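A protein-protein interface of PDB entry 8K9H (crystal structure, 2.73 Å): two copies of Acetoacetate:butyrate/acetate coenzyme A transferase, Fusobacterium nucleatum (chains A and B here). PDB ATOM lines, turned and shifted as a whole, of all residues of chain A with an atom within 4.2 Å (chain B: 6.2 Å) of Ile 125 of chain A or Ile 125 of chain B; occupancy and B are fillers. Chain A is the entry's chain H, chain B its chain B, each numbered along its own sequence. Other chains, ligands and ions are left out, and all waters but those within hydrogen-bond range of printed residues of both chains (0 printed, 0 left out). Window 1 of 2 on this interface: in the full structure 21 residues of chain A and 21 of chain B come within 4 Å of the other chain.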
ATOM      1  N   GLU A 113      27.536  27.965  17.231  1.00  0.00           N
ATOM      2  CA  GLU A 113      27.881  27.128  18.371  1.00  0.00           C
ATOM      3  C   GLU A 113      29.333  27.306  18.798  1.00  0.00           C
ATOM      4  O   GLU A 113      29.630  27.278  19.996  1.00  0.00           O
ATOM      5  CB  GLU A 113      27.610  25.668  18.037  1.00  0.00           C
ATOM      6  CG  GLU A 113      26.150  25.282  18.149  1.00  0.00           C
ATOM      7  CD  GLU A 113      25.493  25.852  19.389  1.00  0.00           C
ATOM      8  OE1 GLU A 113      26.102  25.773  20.488  1.00  0.00           O
ATOM      9  OE2 GLU A 113      24.365  26.382  19.259  1.00  0.00           O
ATOM     10  N   GLY A 124      34.118  22.725  23.580  1.00  0.00           N
ATOM     11  CA  GLY A 124      33.758  22.259  22.261  1.00  0.00           C
ATOM     12  C   GLY A 124      32.337  21.739  22.265  1.00  0.00           C
ATOM     13  O   GLY A 124      31.739  21.468  23.300  1.00  0.00           O
ATOM     14  N   ILE A 125      31.775  21.603  21.066  1.00  0.00           N
ATOM     15  CA  ILE A 125      30.457  21.009  20.900  1.00  0.00           C
ATOM     16  C   ILE A 125      30.538  19.950  19.815  1.00  0.00           C
ATOM     17  O   ILE A 125      31.434  19.966  18.971  1.00  0.00           O
ATOM     18  CB  ILE A 125      29.367  22.054  20.565  1.00  0.00           C
ATOM     19  CG1 ILE A 125      29.812  22.953  19.395  1.00  0.00           C
ATOM     20  CG2 ILE A 125      29.039  22.868  21.796  1.00  0.00           C
ATOM     21  CD1 ILE A 125      29.204  22.547  18.061  1.00  0.00           C
ATOM     22  N   LEU A 126      29.578  19.026  19.856  1.00  0.00           N
ATOM     23  CA  LEU A 126      29.433  17.948  18.883  1.00  0.00           C
ATOM     24  C   LEU A 126      28.228  18.219  17.992  1.00  0.00           C
ATOM     25  O   LEU A 126      27.088  18.251  18.478  1.00  0.00           O
ATOM     26  CB  LEU A 126      29.239  16.602  19.570  1.00  0.00           C
ATOM     27  CG  LEU A 126      30.221  16.174  20.633  1.00  0.00           C
ATOM     28  CD1 LEU A 126      29.980  14.719  20.869  1.00  0.00           C
ATOM     29  CD2 LEU A 126      31.628  16.408  20.161  1.00  0.00           C
ATOM     30  N   THR A 127      28.470  18.355  16.691  1.00  0.00           N
ATOM     31  CA  THR A 127      27.371  18.558  15.761  1.00  0.00           C
ATOM     32  C   THR A 127      27.358  17.480  14.675  1.00  0.00           C
ATOM     33  O   THR A 127      28.410  16.964  14.291  1.00  0.00           O
ATOM     34  CB  THR A 127      27.478  19.937  15.110  1.00  0.00           C
ATOM     35  OG1 THR A 127      26.470  20.064  14.105  1.00  0.00           O
ATOM     36  CG2 THR A 127      28.839  20.107  14.485  1.00  0.00           C
ATOM     37  N   LEU A 150      30.859  15.636  14.821  1.00  0.00           N
ATOM     38  CA  LEU A 150      32.061  16.428  14.637  1.00  0.00           C
ATOM     39  C   LEU A 150      32.310  17.229  15.904  1.00  0.00           C
ATOM     40  O   LEU A 150      31.429  17.972  16.351  1.00  0.00           O
ATOM     41  CB  LEU A 150      31.907  17.377  13.446  1.00  0.00           C
ATOM     42  CG  LEU A 150      32.038  16.803  12.033  1.00  0.00           C
ATOM     43  CD1 LEU A 150      32.183  17.931  11.026  1.00  0.00           C
ATOM     44  CD2 LEU A 150      33.231  15.843  11.941  1.00  0.00           C
ATOM     45  N   LEU A 151      33.492  17.068  16.486  1.00  0.00           N
ATOM     46  CA  LEU A 151      33.947  17.991  17.515  1.00  0.00           C
ATOM     47  C   LEU A 151      34.295  19.324  16.867  1.00  0.00           C
ATOM     48  O   LEU A 151      35.273  19.428  16.113  1.00  0.00           O
ATOM     49  CB  LEU A 151      35.161  17.437  18.249  1.00  0.00           C
ATOM     50  CG  LEU A 151      35.620  18.371  19.366  1.00  0.00           C
ATOM     51  CD1 LEU A 151      34.418  18.709  20.257  1.00  0.00           C
ATOM     52  CD2 LEU A 151      36.716  17.703  20.154  1.00  0.00           C
ATOM     53  N   GLU A 152      33.518  20.353  17.168  1.00  0.00           N
ATOM     54  CA  GLU A 152      33.841  21.699  16.737  1.00  0.00           C
ATOM     55  C   GLU A 152      34.267  22.526  17.948  1.00  0.00           C
ATOM     56  O   GLU A 152      33.616  22.485  19.004  1.00  0.00           O
ATOM     57  CB  GLU A 152      32.654  22.292  15.988  1.00  0.00           C
ATOM     58  CG  GLU A 152      32.263  21.399  14.834  1.00  0.00           C
ATOM     59  CD  GLU A 152      32.858  21.838  13.486  1.00  0.00           C
ATOM     60  OE1 GLU A 152      33.925  22.501  13.480  1.00  0.00           O
ATOM     61  OE2 GLU A 152      32.216  21.537  12.437  1.00  0.00           O
ATOM     62  N   GLY B 109      24.964  23.879  35.514  1.00  0.00           N
ATOM     63  CA  GLY B 109      25.328  24.334  34.185  1.00  0.00           C
ATOM     64  C   GLY B 109      25.419  23.200  33.176  1.00  0.00           C
ATOM     65  O   GLY B 109      25.059  23.357  32.003  1.00  0.00           O
ATOM     66  N   THR B 110      25.939  22.055  33.610  1.00  0.00           N
ATOM     67  CA  THR B 110      25.938  20.889  32.756  1.00  0.00           C
ATOM     68  C   THR B 110      24.513  20.489  32.430  1.00  0.00           C
ATOM     69  O   THR B 110      24.202  20.142  31.283  1.00  0.00           O
ATOM     70  CB  THR B 110      26.695  19.761  33.445  1.00  0.00           C
ATOM     71  OG1 THR B 110      28.078  20.105  33.503  1.00  0.00           O
ATOM     72  CG2 THR B 110      26.528  18.451  32.717  1.00  0.00           C
ATOM     73  N   GLU B 113      23.206  22.759  29.630  1.00  0.00           N
ATOM     74  CA  GLU B 113      23.757  22.381  28.336  1.00  0.00           C
ATOM     75  C   GLU B 113      23.267  20.996  27.887  1.00  0.00           C
ATOM     76  O   GLU B 113      23.062  20.769  26.686  1.00  0.00           O
ATOM     77  CB  GLU B 113      25.280  22.451  28.396  1.00  0.00           C
ATOM     78  CG  GLU B 113      25.828  23.879  28.552  1.00  0.00           C
ATOM     79  CD  GLU B 113      25.393  24.849  27.437  1.00  0.00           C
ATOM     80  OE1 GLU B 113      25.476  24.498  26.238  1.00  0.00           O
ATOM     81  OE2 GLU B 113      24.962  25.978  27.761  1.00  0.00           O
ATOM     82  N   ARG B 114      23.027  20.070  28.823  1.00  0.00           N
ATOM     83  CA  ARG B 114      22.577  18.748  28.418  1.00  0.00           C
ATOM     84  C   ARG B 114      21.139  18.780  27.904  1.00  0.00           C
ATOM     85  O   ARG B 114      20.835  18.195  26.856  1.00  0.00           O
ATOM     86  CB  ARG B 114      22.735  17.767  29.571  1.00  0.00           C
ATOM     87  CG  ARG B 114      24.171  17.351  29.766  1.00  0.00           C
ATOM     88  CD  ARG B 114      24.306  16.316  30.843  1.00  0.00           C
ATOM     89  NE  ARG B 114      23.754  15.044  30.403  1.00  0.00           N
ATOM     90  CZ  ARG B 114      23.528  14.013  31.207  1.00  0.00           C
ATOM     91  NH1 ARG B 114      23.794  14.117  32.504  1.00  0.00           N
ATOM     92  NH2 ARG B 114      23.037  12.886  30.712  1.00  0.00           N
ATOM     93  N   ALA B 117      21.194  20.604  24.612  1.00  0.00           N
ATOM     94  CA  ALA B 117      21.779  19.866  23.502  1.00  0.00           C
ATOM     95  C   ALA B 117      20.734  18.994  22.834  1.00  0.00           C
ATOM     96  O   ALA B 117      20.705  18.898  21.602  1.00  0.00           O
ATOM     97  CB  ALA B 117      22.972  19.034  23.962  1.00  0.00           C
ATOM     98  N   LEU B 122      22.447  18.978  19.017  1.00  0.00           N
ATOM     99  CA  LEU B 122      23.828  18.691  19.339  1.00  0.00           C
ATOM    100  C   LEU B 122      23.958  17.256  19.832  1.00  0.00           C
ATOM    101  O   LEU B 122      23.018  16.672  20.380  1.00  0.00           O
ATOM    102  CB  LEU B 122      24.330  19.682  20.393  1.00  0.00           C
ATOM    103  CG  LEU B 122      24.317  21.157  19.943  1.00  0.00           C
ATOM    104  CD1 LEU B 122      25.107  22.039  20.870  1.00  0.00           C
ATOM    105  CD2 LEU B 122      24.889  21.298  18.562  1.00  0.00           C
ATOM    106  N   GLY B 123      25.123  16.668  19.598  1.00  0.00           N
ATOM    107  CA  GLY B 123      25.337  15.313  20.064  1.00  0.00           C
ATOM    108  C   GLY B 123      25.914  15.214  21.446  1.00  0.00           C
ATOM    109  O   GLY B 123      25.994  14.110  21.994  1.00  0.00           O
ATOM    110  N   GLY B 124      26.294  16.351  22.014  1.00  0.00           N
ATOM    111  CA  GLY B 124      26.963  16.445  23.296  1.00  0.00           C
ATOM    112  C   GLY B 124      27.694  17.763  23.406  1.00  0.00           C
ATOM    113  O   GLY B 124      27.850  18.494  22.437  1.00  0.00           O
ATOM    114  N   ILE B 125      28.142  18.073  24.619  1.00  0.00           N
ATOM    115  CA  ILE B 125      28.923  19.284  24.845  1.00  0.00           C
ATOM    116  C   ILE B 125      30.116  18.941  25.729  1.00  0.00           C
ATOM    117  O   ILE B 125      30.065  18.007  26.538  1.00  0.00           O
ATOM    118  CB  ILE B 125      28.068  20.414  25.471  1.00  0.00           C
ATOM    119  CG1 ILE B 125      27.308  19.908  26.686  1.00  0.00           C
ATOM    120  CG2 ILE B 125      27.060  20.948  24.483  1.00  0.00           C
ATOM    121  CD1 ILE B 125      28.021  20.208  27.958  1.00  0.00           C
ATOM    122  N   LEU B 126      31.198  19.706  25.571  1.00  0.00           N
ATOM    123  CA  LEU B 126      32.417  19.517  26.358  1.00  0.00           C
ATOM    124  C   LEU B 126      32.473  20.541  27.492  1.00  0.00           C
ATOM    125  O   LEU B 126      32.583  21.744  27.228  1.00  0.00           O
ATOM    126  CB  LEU B 126      33.665  19.650  25.479  1.00  0.00           C
ATOM    127  CG  LEU B 126      33.849  18.722  24.274  1.00  0.00           C
ATOM    128  CD1 LEU B 126      35.328  18.592  23.945  1.00  0.00           C
ATOM    129  CD2 LEU B 126      33.244  17.361  24.521  1.00  0.00           C
ATOM    130  N   THR B 127      32.436  20.068  28.753  1.00  0.00           N
ATOM    131  CA  THR B 127      32.488  21.012  29.884  1.00  0.00           C
ATOM    132  C   THR B 127      33.639  20.681  30.828  1.00  0.00           C
ATOM    133  O   THR B 127      33.946  19.506  31.037  1.00  0.00           O
ATOM    134  CB  THR B 127      31.162  21.043  30.697  1.00  0.00           C
ATOM    135  OG1 THR B 127      31.323  21.883  31.846  1.00  0.00           O
ATOM    136  CG2 THR B 127      30.738  19.669  31.140  1.00  0.00           C
ATOM    137  N   LEU B 150      34.810  17.083  30.038  1.00  0.00           N
ATOM    138  CA  LEU B 150      33.871  15.977  30.139  1.00  0.00           C
ATOM    139  C   LEU B 150      32.922  16.044  28.953  1.00  0.00           C
ATOM    140  O   LEU B 150      32.423  17.122  28.609  1.00  0.00           O
ATOM    141  CB  LEU B 150      33.080  16.009  31.457  1.00  0.00           C
ATOM    142  CG  LEU B 150      33.800  15.975  32.809  1.00  0.00           C
ATOM    143  CD1 LEU B 150      32.793  15.806  33.898  1.00  0.00           C
ATOM    144  CD2 LEU B 150      34.830  14.878  32.900  1.00  0.00           C
ATOM    145  N   LEU B 151      32.688  14.899  28.323  1.00  0.00           N
ATOM    146  CA  LEU B 151      31.629  14.794  27.334  1.00  0.00           C
ATOM    147  C   LEU B 151      30.313  14.580  28.071  1.00  0.00           C
ATOM    148  O   LEU B 151      30.078  13.511  28.642  1.00  0.00           O
ATOM    149  CB  LEU B 151      31.914  13.656  26.363  1.00  0.00           C
ATOM    150  CG  LEU B 151      30.810  13.370  25.334  1.00  0.00           C
ATOM    151  CD1 LEU B 151      30.359  14.635  24.635  1.00  0.00           C
ATOM    152  CD2 LEU B 151      31.328  12.358  24.333  1.00  0.00           C
ATOM    153  N   GLU B 152      29.461  15.594  28.073  1.00  0.00           N
ATOM    154  CA  GLU B 152      28.110  15.483  28.607  1.00  0.00           C
ATOM    155  C   GLU B 152      27.136  15.377  27.451  1.00  0.00           C
ATOM    156  O   GLU B 152      27.237  16.136  26.485  1.00  0.00           O
ATOM    157  CB  GLU B 152      27.773  16.683  29.486  1.00  0.00           C
ATOM    158  CG  GLU B 152      28.747  16.819  30.652  1.00  0.00           C
ATOM    159  CD  GLU B 152      28.541  15.754  31.733  1.00  0.00           C
ATOM    160  OE1 GLU B 152      27.625  14.901  31.594  1.00  0.00           O
ATOM    161  OE2 GLU B 152      29.284  15.789  32.737  1.00  0.00           O
ATOM    162  N   LYS B 153      26.170  14.423  27.566  1.00  0.00           N
ATOM    163  CA  LYS B 153      25.269  13.860  26.569  1.00  0.00           C
ATOM    164  C   LYS B 153      23.890  14.525  26.604  1.00  0.00           C
ATOM    165  O   LYS B 153      23.400  14.932  27.668  1.00  0.00           O
ATOM    166  CB  LYS B 153      25.125  12.348  26.797  1.00  0.00           C
ATOM    167  CG  LYS B 153      26.422  11.561  26.535  1.00  0.00           C
ATOM    168  CD  LYS B 153      26.228  10.043  26.568  1.00  0.00           C
ATOM    169  CE  LYS B 153      25.104   9.659  27.528  1.00  0.00           C
ATOM    170  NZ  LYS B 153      24.762   8.209  27.448  1.00  0.00           N
ATOM    171  N   PRO B 154      23.221  14.627  25.456  1.00  0.00           N
ATOM    172  CA  PRO B 154      21.899  15.256  25.432  1.00  0.00           C
ATOM    173  C   PRO B 154      20.896  14.459  26.241  1.00  0.00           C
ATOM    174  O   PRO B 154      21.052  13.262  26.484  1.00  0.00           O
ATOM    175  CB  PRO B 154      21.525  15.261  23.945  1.00  0.00           C
ATOM    176  CG  PRO B 154      22.756  14.932  23.232  1.00  0.00           C
ATOM    177  CD  PRO B 154      23.585  14.099  24.139  1.00  0.00           C
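The backbone NH (N) of Gly 123 of chain B is in hydrogen-bond range of the backbone carbonyl oxygen (O) of Leu 126 of chain A.
The backbone NH (N) of Leu 126 of chain B sits at hydrogen-bond distance from the backbone carbonyl oxygen (O) of Gly 124 of chain A, 2.9 Å away.
O of Gly 124 of chain B is in hydrogen-bond range of N of Leu 126 of chain A.
N of Ile 125 of chain B lies within hydrogen-bond range of O of Glu 152 of chain B (2.8 Å).
The backbone carbonyl oxygen (O) of Ala 117 of chain B sits at hydrogen-bond distance from the backbone NH (N) of Leu 122 of chain B, 3.1 Å away.
N of Glu 152 of chain A sits at hydrogen-bond distance from O of Ile 125 of chain A (2.8 Å).
OE1 of Glu 113 of chain A touches CD1 of Leu 122 of chain B (3.9 Å).
Ile 125 of chain B touches Gly 124 of chain A.
CA of Ile 125 of chain A touches O of Gly 124 of chain B, 3.9 Å away.
Ile 125 of chain A touches Ile 125 of chain B.
Leu 122 of chain B touches Leu 126 of chain A.
Leu 126 of chain A touches Leu 151 of chain B.
CD1 of Leu 151 of chain A touches CD1 of Leu 126 of chain B, 3.8 Å away.
Of the printed residues of chain B, Ile 125 of chain A touches Gly 124 (3.9 Å) and Ile 125 (3.9 Å).
Glu 152 of chain A touches none of the printed residues of chain B.
Of the printed residues of chain A, Leu 122 of chain B touches Glu 113 (3.9 Å) and Leu 126 (3.4 Å).
Printed residues of chain A within 4 Å of Gly 123 of chain B: Leu 126.
Of the printed residues of chain A, Gly 124 of chain B touches Ile 125 (3.9 Å) and Leu 126 (3.2 Å).
Ile 125 of chain B touches just these residues of chain A: Gly 124 and Ile 125.
Printed residues of chain A within 4 Å of Leu 126 of chain B: Gly 124 (2.9 Å) and Leu 151 (3.8 Å).
The nearest residue of chain B that does not touch Ile 125 of chain A is Leu 122 of chain B (4.1 Å).
Hydrophobic or aromatic side chains of chain A that line the printed part of chain B: Ile 125, Leu 126 and Leu 151.
Among the printed residues, 10 pairs touch across the chains.
Among the printed residues, no Asp or Glu carboxylate lies within 4 Å of a Lys or Arg side-chain nitrogen of the other chain.
Gly 124 of chain A touches Ile 125 of chain B, and with the chains exchanged Ile 125 of chain A touches Gly 124 of chain B.
Gly 124 of chain A touches Leu 126 of chain B, and with the chains exchanged Leu 126 of chain A touches Gly 124 of chain B.
Ile 125 of chain B touches its own counterpart, Ile 125 of chain A.
Leu 126 of chain A touches Leu 151 of chain B, and with the chains exchanged Leu 151 of chain A touches Leu 126 of chain B.
Positions printed for both chains: 113, 124, 125, 126, 127, 150, 151 and 152.
Of the 10 pairs that touch across the chains among the printed residues, 7 have their exchanged pair printed and touching as well.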
